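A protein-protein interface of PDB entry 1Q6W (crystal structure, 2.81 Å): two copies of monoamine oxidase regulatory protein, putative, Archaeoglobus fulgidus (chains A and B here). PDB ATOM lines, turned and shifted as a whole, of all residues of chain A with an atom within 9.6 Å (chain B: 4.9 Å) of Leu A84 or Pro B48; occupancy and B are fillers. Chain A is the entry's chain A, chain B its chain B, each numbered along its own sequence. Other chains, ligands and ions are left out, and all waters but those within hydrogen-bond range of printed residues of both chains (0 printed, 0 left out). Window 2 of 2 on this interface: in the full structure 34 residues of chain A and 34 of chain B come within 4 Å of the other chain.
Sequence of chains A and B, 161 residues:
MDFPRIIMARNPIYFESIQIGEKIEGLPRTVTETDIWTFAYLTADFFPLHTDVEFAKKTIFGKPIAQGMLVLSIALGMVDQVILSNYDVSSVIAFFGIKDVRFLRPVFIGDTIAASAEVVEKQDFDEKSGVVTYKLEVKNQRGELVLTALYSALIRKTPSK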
ATOM      1  N   ALA A   9     -10.916  -5.322  20.058  1.00  0.00           N
ATOM      2  CA  ALA A   9     -11.511  -4.180  19.292  1.00  0.00           C
ATOM      3  C   ALA A   9     -10.534  -2.996  19.137  1.00  0.00           C
ATOM      4  O   ALA A   9      -9.944  -2.533  20.114  1.00  0.00           O
ATOM      5  CB  ALA A   9     -12.786  -3.726  19.990  1.00  0.00           C
ATOM      6  N   ARG A  10     -10.365  -2.502  17.913  1.00  0.00           N
ATOM      7  CA  ARG A  10      -9.443  -1.384  17.657  1.00  0.00           C
ATOM      8  C   ARG A  10     -10.119  -0.020  17.877  1.00  0.00           C
ATOM      9  O   ARG A  10     -10.384   0.381  19.018  1.00  0.00           O
ATOM     10  CB  ARG A  10      -8.913  -1.437  16.212  1.00  0.00           C
ATOM     11  CG  ARG A  10      -8.364  -2.788  15.725  1.00  0.00           C
ATOM     12  CD  ARG A  10      -8.032  -2.700  14.225  1.00  0.00           C
ATOM     13  NE  ARG A  10      -7.827  -3.987  13.550  1.00  0.00           N
ATOM     14  CZ  ARG A  10      -6.762  -4.771  13.707  1.00  0.00           C
ATOM     15  NH1 ARG A  10      -5.783  -4.415  14.529  1.00  0.00           N
ATOM     16  NH2 ARG A  10      -6.667  -5.908  13.025  1.00  0.00           N
ATOM     17  N   ASN A  11     -10.384   0.687  16.772  1.00  0.00           N
ATOM     18  CA  ASN A  11     -11.035   2.001  16.803  1.00  0.00           C
ATOM     19  C   ASN A  11     -12.390   1.921  16.124  1.00  0.00           C
ATOM     20  O   ASN A  11     -12.618   1.051  15.289  1.00  0.00           O
ATOM     21  CB  ASN A  11     -10.179   3.044  16.087  1.00  0.00           C
ATOM     22  CG  ASN A  11      -8.891   3.339  16.821  1.00  0.00           C
ATOM     23  OD1 ASN A  11      -8.897   3.939  17.899  1.00  0.00           O
ATOM     24  ND2 ASN A  11      -7.774   2.909  16.247  1.00  0.00           N
ATOM     25  N   ILE A  13     -15.621   2.576  13.657  1.00  0.00           N
ATOM     26  CA  ILE A  13     -15.759   2.817  12.231  1.00  0.00           C
ATOM     27  C   ILE A  13     -17.022   3.617  12.005  1.00  0.00           C
ATOM     28  O   ILE A  13     -18.092   3.230  12.452  1.00  0.00           O
ATOM     29  CB  ILE A  13     -15.880   1.508  11.423  1.00  0.00           C
ATOM     30  CG1 ILE A  13     -16.838   0.548  12.133  1.00  0.00           C
ATOM     31  CG2 ILE A  13     -14.506   0.910  11.199  1.00  0.00           C
ATOM     32  CD1 ILE A  13     -17.144  -0.703  11.337  1.00  0.00           C
ATOM     33  N   ILE A  24     -16.054  -9.143   4.329  1.00  0.00           N
ATOM     34  CA  ILE A  24     -15.707  -9.760   5.602  1.00  0.00           C
ATOM     35  C   ILE A  24     -15.820 -11.272   5.459  1.00  0.00           C
ATOM     36  O   ILE A  24     -16.833 -11.779   4.983  1.00  0.00           O
ATOM     37  CB  ILE A  24     -16.652  -9.299   6.725  1.00  0.00           C
ATOM     38  CG1 ILE A  24     -16.548  -7.786   6.897  1.00  0.00           C
ATOM     39  CG2 ILE A  24     -16.285  -9.982   8.024  1.00  0.00           C
ATOM     40  CD1 ILE A  24     -17.607  -7.204   7.796  1.00  0.00           C
ATOM     41  N   LEU A  76     -24.734 -14.665   9.965  1.00  0.00           N
ATOM     42  CA  LEU A  76     -24.610 -13.298  10.442  1.00  0.00           C
ATOM     43  C   LEU A  76     -23.690 -13.260  11.663  1.00  0.00           C
ATOM     44  O   LEU A  76     -22.895 -12.341  11.840  1.00  0.00           O
ATOM     45  CB  LEU A  76     -25.974 -12.759  10.807  1.00  0.00           C
ATOM     46  CG  LEU A  76     -26.901 -12.553   9.601  1.00  0.00           C
ATOM     47  CD1 LEU A  76     -28.319 -12.193  10.058  1.00  0.00           C
ATOM     48  CD2 LEU A  76     -26.316 -11.452   8.682  1.00  0.00           C
ATOM     49  N   GLY A  77     -23.785 -14.301  12.482  1.00  0.00           N
ATOM     50  CA  GLY A  77     -22.987 -14.382  13.676  1.00  0.00           C
ATOM     51  C   GLY A  77     -21.510 -14.473  13.425  1.00  0.00           C
ATOM     52  O   GLY A  77     -20.748 -13.730  14.028  1.00  0.00           O
ATOM     53  N   MET A  78     -21.079 -15.368  12.549  1.00  0.00           N
ATOM     54  CA  MET A  78     -19.655 -15.487  12.328  1.00  0.00           C
ATOM     55  C   MET A  78     -19.069 -14.273  11.614  1.00  0.00           C
ATOM     56  O   MET A  78     -17.867 -14.016  11.691  1.00  0.00           O
ATOM     57  CB  MET A  78     -19.313 -16.802  11.615  1.00  0.00           C
ATOM     58  CG  MET A  78     -20.035 -17.066  10.310  1.00  0.00           C
ATOM     59  SD  MET A  78     -19.644 -18.849   9.606  1.00  0.00           S
ATOM     60  CE  MET A  78     -21.422 -19.577   9.569  1.00  0.00           C
ATOM     61  N   VAL A  79     -19.921 -13.503  10.948  1.00  0.00           N
ATOM     62  CA  VAL A  79     -19.467 -12.297  10.256  1.00  0.00           C
ATOM     63  C   VAL A  79     -19.290 -11.185  11.274  1.00  0.00           C
ATOM     64  O   VAL A  79     -18.309 -10.443  11.229  1.00  0.00           O
ATOM     65  CB  VAL A  79     -20.493 -11.837   9.168  1.00  0.00           C
ATOM     66  CG1 VAL A  79     -20.325 -10.366   8.854  1.00  0.00           C
ATOM     67  CG2 VAL A  79     -20.278 -12.654   7.891  1.00  0.00           C
ATOM     68  N   ASP A  80     -20.248 -11.075  12.194  1.00  0.00           N
ATOM     69  CA  ASP A  80     -20.192 -10.053  13.224  1.00  0.00           C
ATOM     70  C   ASP A  80     -19.012 -10.300  14.165  1.00  0.00           C
ATOM     71  O   ASP A  80     -18.405  -9.362  14.679  1.00  0.00           O
ATOM     72  CB  ASP A  80     -21.493 -10.025  14.016  1.00  0.00           C
ATOM     73  CG  ASP A  80     -21.663  -8.737  14.800  1.00  0.00           C
ATOM     74  OD1 ASP A  80     -21.643  -7.650  14.186  1.00  0.00           O
ATOM     75  OD2 ASP A  80     -21.820  -8.806  16.035  1.00  0.00           O
ATOM     76  N   GLN A  81     -18.680 -11.568  14.373  1.00  0.00           N
ATOM     77  CA  GLN A  81     -17.568 -11.928  15.236  1.00  0.00           C
ATOM     78  C   GLN A  81     -16.270 -11.272  14.756  1.00  0.00           C
ATOM     79  O   GLN A  81     -15.445 -10.870  15.567  1.00  0.00           O
ATOM     80  CB  GLN A  81     -17.417 -13.445  15.272  1.00  0.00           C
ATOM     81  CG  GLN A  81     -16.728 -13.959  16.513  1.00  0.00           C
ATOM     82  CD  GLN A  81     -16.792 -15.469  16.616  1.00  0.00           C
ATOM     83  OE1 GLN A  81     -17.844 -16.067  16.415  1.00  0.00           O
ATOM     84  NE2 GLN A  81     -15.665 -16.093  16.933  1.00  0.00           N
ATOM     85  N   VAL A  82     -16.099 -11.163  13.442  1.00  0.00           N
ATOM     86  CA  VAL A  82     -14.905 -10.539  12.888  1.00  0.00           C
ATOM     87  C   VAL A  82     -14.905  -9.025  13.135  1.00  0.00           C
ATOM     88  O   VAL A  82     -13.876  -8.438  13.486  1.00  0.00           O
ATOM     89  CB  VAL A  82     -14.787 -10.786  11.379  1.00  0.00           C
ATOM     90  CG1 VAL A  82     -13.638 -10.000  10.814  1.00  0.00           C
ATOM     91  CG2 VAL A  82     -14.573 -12.257  11.118  1.00  0.00           C
ATOM     92  N   ILE A  83     -16.059  -8.391  12.952  1.00  0.00           N
ATOM     93  CA  ILE A  83     -16.163  -6.954  13.173  1.00  0.00           C
ATOM     94  C   ILE A  83     -15.916  -6.659  14.645  1.00  0.00           C
ATOM     95  O   ILE A  83     -15.142  -5.775  14.999  1.00  0.00           O
ATOM     96  CB  ILE A  83     -17.556  -6.440  12.760  1.00  0.00           C
ATOM     97  CG1 ILE A  83     -17.710  -6.547  11.241  1.00  0.00           C
ATOM     98  CG2 ILE A  83     -17.735  -5.014  13.202  1.00  0.00           C
ATOM     99  CD1 ILE A  83     -19.094  -6.186  10.750  1.00  0.00           C
ATOM    100  N   LEU A  84     -16.579  -7.427  15.498  1.00  0.00           N
ATOM    101  CA  LEU A  84     -16.473  -7.304  16.948  1.00  0.00           C
ATOM    102  C   LEU A  84     -15.047  -7.351  17.483  1.00  0.00           C
ATOM    103  O   LEU A  84     -14.733  -6.702  18.487  1.00  0.00           O
ATOM    104  CB  LEU A  84     -17.255  -8.426  17.604  1.00  0.00           C
ATOM    105  CG  LEU A  84     -18.456  -8.063  18.457  1.00  0.00           C
ATOM    106  CD1 LEU A  84     -19.078  -6.752  17.985  1.00  0.00           C
ATOM    107  CD2 LEU A  84     -19.446  -9.242  18.378  1.00  0.00           C
ATOM    108  N   SER A  85     -14.179  -8.123  16.838  1.00  0.00           N
ATOM    109  CA  SER A  85     -12.815  -8.212  17.324  1.00  0.00           C
ATOM    110  C   SER A  85     -11.830  -7.320  16.591  1.00  0.00           C
ATOM    111  O   SER A  85     -10.628  -7.425  16.795  1.00  0.00           O
ATOM    112  CB  SER A  85     -12.345  -9.663  17.301  1.00  0.00           C
ATOM    113  OG  SER A  85     -12.737 -10.275  16.101  1.00  0.00           O
ATOM    114  N   ASN A  86     -12.335  -6.430  15.750  1.00  0.00           N
ATOM    115  CA  ASN A  86     -11.462  -5.522  15.022  1.00  0.00           C
ATOM    116  C   ASN A  86     -11.876  -4.062  15.096  1.00  0.00           C
ATOM    117  O   ASN A  86     -11.095  -3.183  14.730  1.00  0.00           O
ATOM    118  CB  ASN A  86     -11.355  -5.921  13.552  1.00  0.00           C
ATOM    119  CG  ASN A  86     -10.457  -7.106  13.342  1.00  0.00           C
ATOM    120  OD1 ASN A  86     -10.858  -8.247  13.554  1.00  0.00           O
ATOM    121  ND2 ASN A  86      -9.221  -6.845  12.930  1.00  0.00           N
ATOM    122  N   TYR A  87     -13.092  -3.788  15.562  1.00  0.00           N
ATOM    123  CA  TYR A  87     -13.554  -2.401  15.642  1.00  0.00           C
ATOM    124  C   TYR A  87     -14.355  -2.108  16.879  1.00  0.00           C
ATOM    125  O   TYR A  87     -14.869  -3.022  17.529  1.00  0.00           O
ATOM    126  CB  TYR A  87     -14.422  -2.065  14.442  1.00  0.00           C
ATOM    127  CG  TYR A  87     -13.740  -2.244  13.119  1.00  0.00           C
ATOM    128  CD1 TYR A  87     -12.784  -1.330  12.680  1.00  0.00           C
ATOM    129  CD2 TYR A  87     -14.058  -3.323  12.293  1.00  0.00           C
ATOM    130  CE1 TYR A  87     -12.163  -1.480  11.445  1.00  0.00           C
ATOM    131  CE2 TYR A  87     -13.438  -3.487  11.054  1.00  0.00           C
ATOM    132  CZ  TYR A  87     -12.493  -2.559  10.638  1.00  0.00           C
ATOM    133  OH  TYR A  87     -11.882  -2.704   9.421  1.00  0.00           O
ATOM    134  N   ASP A  88     -14.454  -0.826  17.200  1.00  0.00           N
ATOM    135  CA  ASP A  88     -15.249  -0.393  18.333  1.00  0.00           C
ATOM    136  C   ASP A  88     -16.611  -0.208  17.688  1.00  0.00           C
ATOM    137  O   ASP A  88     -16.824   0.729  16.923  1.00  0.00           O
ATOM    138  CB  ASP A  88     -14.729   0.935  18.892  1.00  0.00           C
ATOM    139  CG  ASP A  88     -15.615   1.495  19.992  1.00  0.00           C
ATOM    140  OD1 ASP A  88     -15.205   2.481  20.638  1.00  0.00           O
ATOM    141  OD2 ASP A  88     -16.722   0.958  20.206  1.00  0.00           O
ATOM    142  N   VAL A  89     -17.526  -1.110  17.985  1.00  0.00           N
ATOM    143  CA  VAL A  89     -18.844  -1.053  17.377  1.00  0.00           C
ATOM    144  C   VAL A  89     -19.843  -0.082  18.017  1.00  0.00           C
ATOM    145  O   VAL A  89     -21.044  -0.206  17.803  1.00  0.00           O
ATOM    146  CB  VAL A  89     -19.461  -2.472  17.317  1.00  0.00           C
ATOM    147  CG1 VAL A  89     -18.504  -3.390  16.574  1.00  0.00           C
ATOM    148  CG2 VAL A  89     -19.743  -3.009  18.756  1.00  0.00           C
ATOM    149  N   SER A  90     -19.359   0.888  18.784  1.00  0.00           N
ATOM    150  CA  SER A  90     -20.268   1.857  19.398  1.00  0.00           C
ATOM    151  C   SER A  90     -20.950   2.695  18.319  1.00  0.00           C
ATOM    152  O   SER A  90     -21.995   3.296  18.558  1.00  0.00           O
ATOM    153  CB  SER A  90     -19.530   2.780  20.375  1.00  0.00           C
ATOM    154  OG  SER A  90     -18.389   3.348  19.781  1.00  0.00           O
ATOM    155  N   SER A  91     -20.362   2.727  17.126  1.00  0.00           N
ATOM    156  CA  SER A  91     -20.928   3.490  16.011  1.00  0.00           C
ATOM    157  C   SER A  91     -22.018   2.710  15.275  1.00  0.00           C
ATOM    158  O   SER A  91     -22.746   3.271  14.455  1.00  0.00           O
ATOM    159  CB  SER A  91     -19.833   3.872  15.032  1.00  0.00           C
ATOM    160  OG  SER A  91     -19.083   2.729  14.680  1.00  0.00           O
ATOM    161  N   VAL A  92     -22.120   1.408  15.558  1.00  0.00           N
ATOM    162  CA  VAL A  92     -23.139   0.573  14.942  1.00  0.00           C
ATOM    163  C   VAL A  92     -24.385   0.777  15.790  1.00  0.00           C
ATOM    164  O   VAL A  92     -24.540   0.161  16.838  1.00  0.00           O
ATOM    165  CB  VAL A  92     -22.746  -0.918  14.951  1.00  0.00           C
ATOM    166  CG1 VAL A  92     -23.797  -1.734  14.231  1.00  0.00           C
ATOM    167  CG2 VAL A  92     -21.404  -1.110  14.269  1.00  0.00           C
ATOM    168  N   ASP B  45     -22.032 -14.986  18.780  1.00  0.00           N
ATOM    169  CA  ASP B  45     -22.051 -13.556  18.512  1.00  0.00           C
ATOM    170  C   ASP B  45     -22.428 -12.757  19.763  1.00  0.00           C
ATOM    171  O   ASP B  45     -23.589 -12.673  20.136  1.00  0.00           O
ATOM    172  CB  ASP B  45     -23.047 -13.282  17.378  1.00  0.00           C
ATOM    173  CG  ASP B  45     -23.241 -11.807  17.107  1.00  0.00           C
ATOM    174  OD1 ASP B  45     -24.132 -11.468  16.299  1.00  0.00           O
ATOM    175  OD2 ASP B  45     -22.510 -10.987  17.695  1.00  0.00           O
ATOM    176  N   PHE B  46     -21.442 -12.154  20.402  1.00  0.00           N
ATOM    177  CA  PHE B  46     -21.706 -11.381  21.597  1.00  0.00           C
ATOM    178  C   PHE B  46     -21.637  -9.880  21.359  1.00  0.00           C
ATOM    179  O   PHE B  46     -20.771  -9.195  21.910  1.00  0.00           O
ATOM    180  CB  PHE B  46     -20.727 -11.770  22.705  1.00  0.00           C
ATOM    181  CG  PHE B  46     -21.133 -12.992  23.466  1.00  0.00           C
ATOM    182  CD1 PHE B  46     -21.009 -14.264  22.904  1.00  0.00           C
ATOM    183  CD2 PHE B  46     -21.711 -12.876  24.727  1.00  0.00           C
ATOM    184  CE1 PHE B  46     -21.462 -15.398  23.594  1.00  0.00           C
ATOM    185  CE2 PHE B  46     -22.170 -14.012  25.423  1.00  0.00           C
ATOM    186  CZ  PHE B  46     -22.043 -15.263  24.854  1.00  0.00           C
ATOM    187  N   PHE B  47     -22.541  -9.372  20.528  1.00  0.00           N
ATOM    188  CA  PHE B  47     -22.604  -7.946  20.246  1.00  0.00           C
ATOM    189  C   PHE B  47     -22.970  -7.258  21.579  1.00  0.00           C
ATOM    190  O   PHE B  47     -24.023  -7.527  22.175  1.00  0.00           O
ATOM    191  CB  PHE B  47     -23.666  -7.669  19.185  1.00  0.00           C
ATOM    192  CG  PHE B  47     -23.600  -6.289  18.614  1.00  0.00           C
ATOM    193  CD1 PHE B  47     -22.607  -5.960  17.696  1.00  0.00           C
ATOM    194  CD2 PHE B  47     -24.496  -5.301  19.028  1.00  0.00           C
ATOM    195  CE1 PHE B  47     -22.495  -4.660  17.192  1.00  0.00           C
ATOM    196  CE2 PHE B  47     -24.394  -3.999  18.535  1.00  0.00           C
ATOM    197  CZ  PHE B  47     -23.384  -3.672  17.608  1.00  0.00           C
ATOM    198  N   PRO B  48     -22.109  -6.336  22.044  1.00  0.00           N
ATOM    199  CA  PRO B  48     -22.286  -5.598  23.299  1.00  0.00           C
ATOM    200  C   PRO B  48     -23.650  -4.990  23.607  1.00  0.00           C
ATOM    201  O   PRO B  48     -24.012  -4.864  24.771  1.00  0.00           O
ATOM    202  CB  PRO B  48     -21.153  -4.566  23.253  1.00  0.00           C
ATOM    203  CG  PRO B  48     -20.967  -4.328  21.809  1.00  0.00           C
ATOM    204  CD  PRO B  48     -21.042  -5.721  21.232  1.00  0.00           C
ATOM    205  N   LEU B  49     -24.415  -4.614  22.589  1.00  0.00           N
ATOM    206  CA  LEU B  49     -25.732  -4.031  22.836  1.00  0.00           C
ATOM    207  C   LEU B  49     -26.637  -5.082  23.485  1.00  0.00           C
ATOM    208  O   LEU B  49     -27.568  -4.744  24.211  1.00  0.00           O
ATOM    209  CB  LEU B  49     -26.374  -3.566  21.528  1.00  0.00           C
ATOM    210  CG  LEU B  49     -27.398  -2.421  21.573  1.00  0.00           C
ATOM    211  CD1 LEU B  49     -28.299  -2.518  20.344  1.00  0.00           C
ATOM    212  CD2 LEU B  49     -28.258  -2.467  22.820  1.00  0.00           C
ATOM    213  N   HIS B  50     -26.350  -6.359  23.232  1.00  0.00           N
ATOM    214  CA  HIS B  50     -27.161  -7.434  23.784  1.00  0.00           C
ATOM    215  C   HIS B  50     -26.548  -8.064  25.012  1.00  0.00           C
ATOM    216  O   HIS B  50     -27.271  -8.453  25.926  1.00  0.00           O
ATOM    217  CB  HIS B  50     -27.367  -8.532  22.746  1.00  0.00           C
ATOM    218  CG  HIS B  50     -27.791  -8.026  21.408  1.00  0.00           C
ATOM    219  ND1 HIS B  50     -28.963  -7.329  21.218  1.00  0.00           N
ATOM    220  CD2 HIS B  50     -27.199  -8.109  20.194  1.00  0.00           C
ATOM    221  CE1 HIS B  50     -29.076  -7.005  19.943  1.00  0.00           C
ATOM    222  NE2 HIS B  50     -28.017  -7.467  19.301  1.00  0.00           N
ATOM    223  N   THR B  51     -25.221  -8.162  25.054  1.00  0.00           N
ATOM    224  CA  THR B  51     -24.595  -8.825  26.184  1.00  0.00           C
ATOM    225  C   THR B  51     -23.568  -8.090  27.030  1.00  0.00           C
ATOM    226  O   THR B  51     -22.797  -8.736  27.745  1.00  0.00           O
ATOM    227  CB  THR B  51     -23.984 -10.139  25.717  1.00  0.00           C
ATOM    228  OG1 THR B  51     -23.108  -9.881  24.614  1.00  0.00           O
ATOM    229  CG2 THR B  51     -25.082 -11.104  25.277  1.00  0.00           C
ATOM    230  N   ASP B  52     -23.553  -6.759  26.947  1.00  0.00           N
ATOM    231  CA  ASP B  52     -22.636  -5.941  27.739  1.00  0.00           C
ATOM    232  C   ASP B  52     -23.439  -4.840  28.452  1.00  0.00           C
ATOM    233  O   ASP B  52     -23.764  -3.792  27.872  1.00  0.00           O
ATOM    234  CB  ASP B  52     -21.567  -5.299  26.850  1.00  0.00           C
ATOM    235  CG  ASP B  52     -20.489  -4.589  27.655  1.00  0.00           C
ATOM    236  OD1 ASP B  52     -20.820  -3.961  28.688  1.00  0.00           O
ATOM    237  OD2 ASP B  52     -19.309  -4.652  27.250  1.00  0.00           O
ATOM    238  N   PHE B  55     -21.942  -1.327  28.156  1.00  0.00           N
ATOM    239  CA  PHE B  55     -22.014  -0.751  26.824  1.00  0.00           C
ATOM    240  C   PHE B  55     -23.417  -0.233  26.502  1.00  0.00           C
ATOM    241  O   PHE B  55     -23.584   0.879  25.980  1.00  0.00           O
ATOM    242  CB  PHE B  55     -21.571  -1.807  25.806  1.00  0.00           C
ATOM    243  CG  PHE B  55     -21.682  -1.371  24.373  1.00  0.00           C
ATOM    244  CD1 PHE B  55     -22.928  -1.323  23.732  1.00  0.00           C
ATOM    245  CD2 PHE B  55     -20.549  -1.076  23.644  1.00  0.00           C
ATOM    246  CE1 PHE B  55     -23.038  -0.993  22.381  1.00  0.00           C
ATOM    247  CE2 PHE B  55     -20.644  -0.739  22.282  1.00  0.00           C
ATOM    248  CZ  PHE B  55     -21.897  -0.700  21.648  1.00  0.00           C
ATOM    249  N   ALA B  56     -24.422  -1.040  26.826  1.00  0.00           N
ATOM    250  CA  ALA B  56     -25.808  -0.677  26.557  1.00  0.00           C
ATOM    251  C   ALA B  56     -26.192   0.666  27.176  1.00  0.00           C
ATOM    252  O   ALA B  56     -26.964   1.433  26.587  1.00  0.00           O
ATOM    253  CB  ALA B  56     -26.728  -1.759  27.067  1.00  0.00           C
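The side-chain carboxylate (OD2) of Asp A80 lies close to the side-chain carboxylate (OD2) of Asp B45, 2.8 Å away.
The side-chain hydroxyl (OG) of Ser A90 is in hydrogen-bond range of the side-chain carboxylate (OD2) of Asp A88 (2.9 Å).
The backbone NH (N) of Phe B47 lies within hydrogen-bond range of the side-chain carboxylate (OD2) of Asp B45 (3.3 Å).
N of Phe B55 is in hydrogen-bond range of OD1 of Asp B52, at 2.9 Å.
Among the printed residues, merely in contact across the chains: Asp A80 with Phe B47 (3.4 Å), Val A89 with Pro B48 (3.5 Å), Val A89 with Phe B47 (3.6 Å), Leu A84 with Asp B45 (3.6 Å), Leu A84 with Phe B47 (3.6 Å), Leu A84 with Phe B46 (3.8 Å), Ser A90 with Phe B55 (3.8 Å), Gly A77 with Asp B45 (3.9 Å), Val A92 with Phe B47 (3.9 Å), Leu A84 with Pro B48 (3.9 Å) and Val A89 with Phe B55 (3.97 Å).
Of chain B, only Asp B45 (3.6 Å), Phe B46 (3.8 Å), Phe B47 (3.6 Å) and Pro B48 (3.9 Å) come within 4 Å of Leu A84.
Of the printed residues of chain A, Pro B48 touches Leu A84 and Val A89.
Phe B47 touches just these residues of chain A: Asp A80 (3.4 Å), Leu A84 (3.6 Å), Val A89 (3.6 Å) and Val A92 (3.9 Å).
No residue of chain A comes within 4 Å of Asp B52.
Printed residues of chain A within 4 Å of Phe B55: Val A89 (3.97 Å) and Ser A90 (3.8 Å).
Of the printed residues of chain A, Phe B46 touches Leu A84 (3.8 Å).
Printed residues of chain B within 4 Å of Val A89: Phe B47 (3.6 Å), Pro B48 (3.5 Å) and Phe B55 (3.97 Å).
Gln A81 touches none of the printed residues of chain B.
Ile A24 touches none of the printed residues of chain B.
The nearest printed residue of chain B that does not touch Asp A80 is Phe B46 (5.4 Å).
Of the 22 printed residues of chain A, 6 touch a printed residue of chain B.
Hydrophobic or aromatic side chains of chain A that line the printed part of chain B: Leu A84, Val A89 and Val A92.
Among the printed residues, 12 pairs touch across the chains.
Among the printed residues, no Asp or Glu carboxylate lies within 4 Å of a Lys or Arg side-chain nitrogen of the other chain.
No position is printed for both chains.
Of the 12 pairs that touch across the chains among the printed residues, none has its exchanged pair printed and touching as well.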
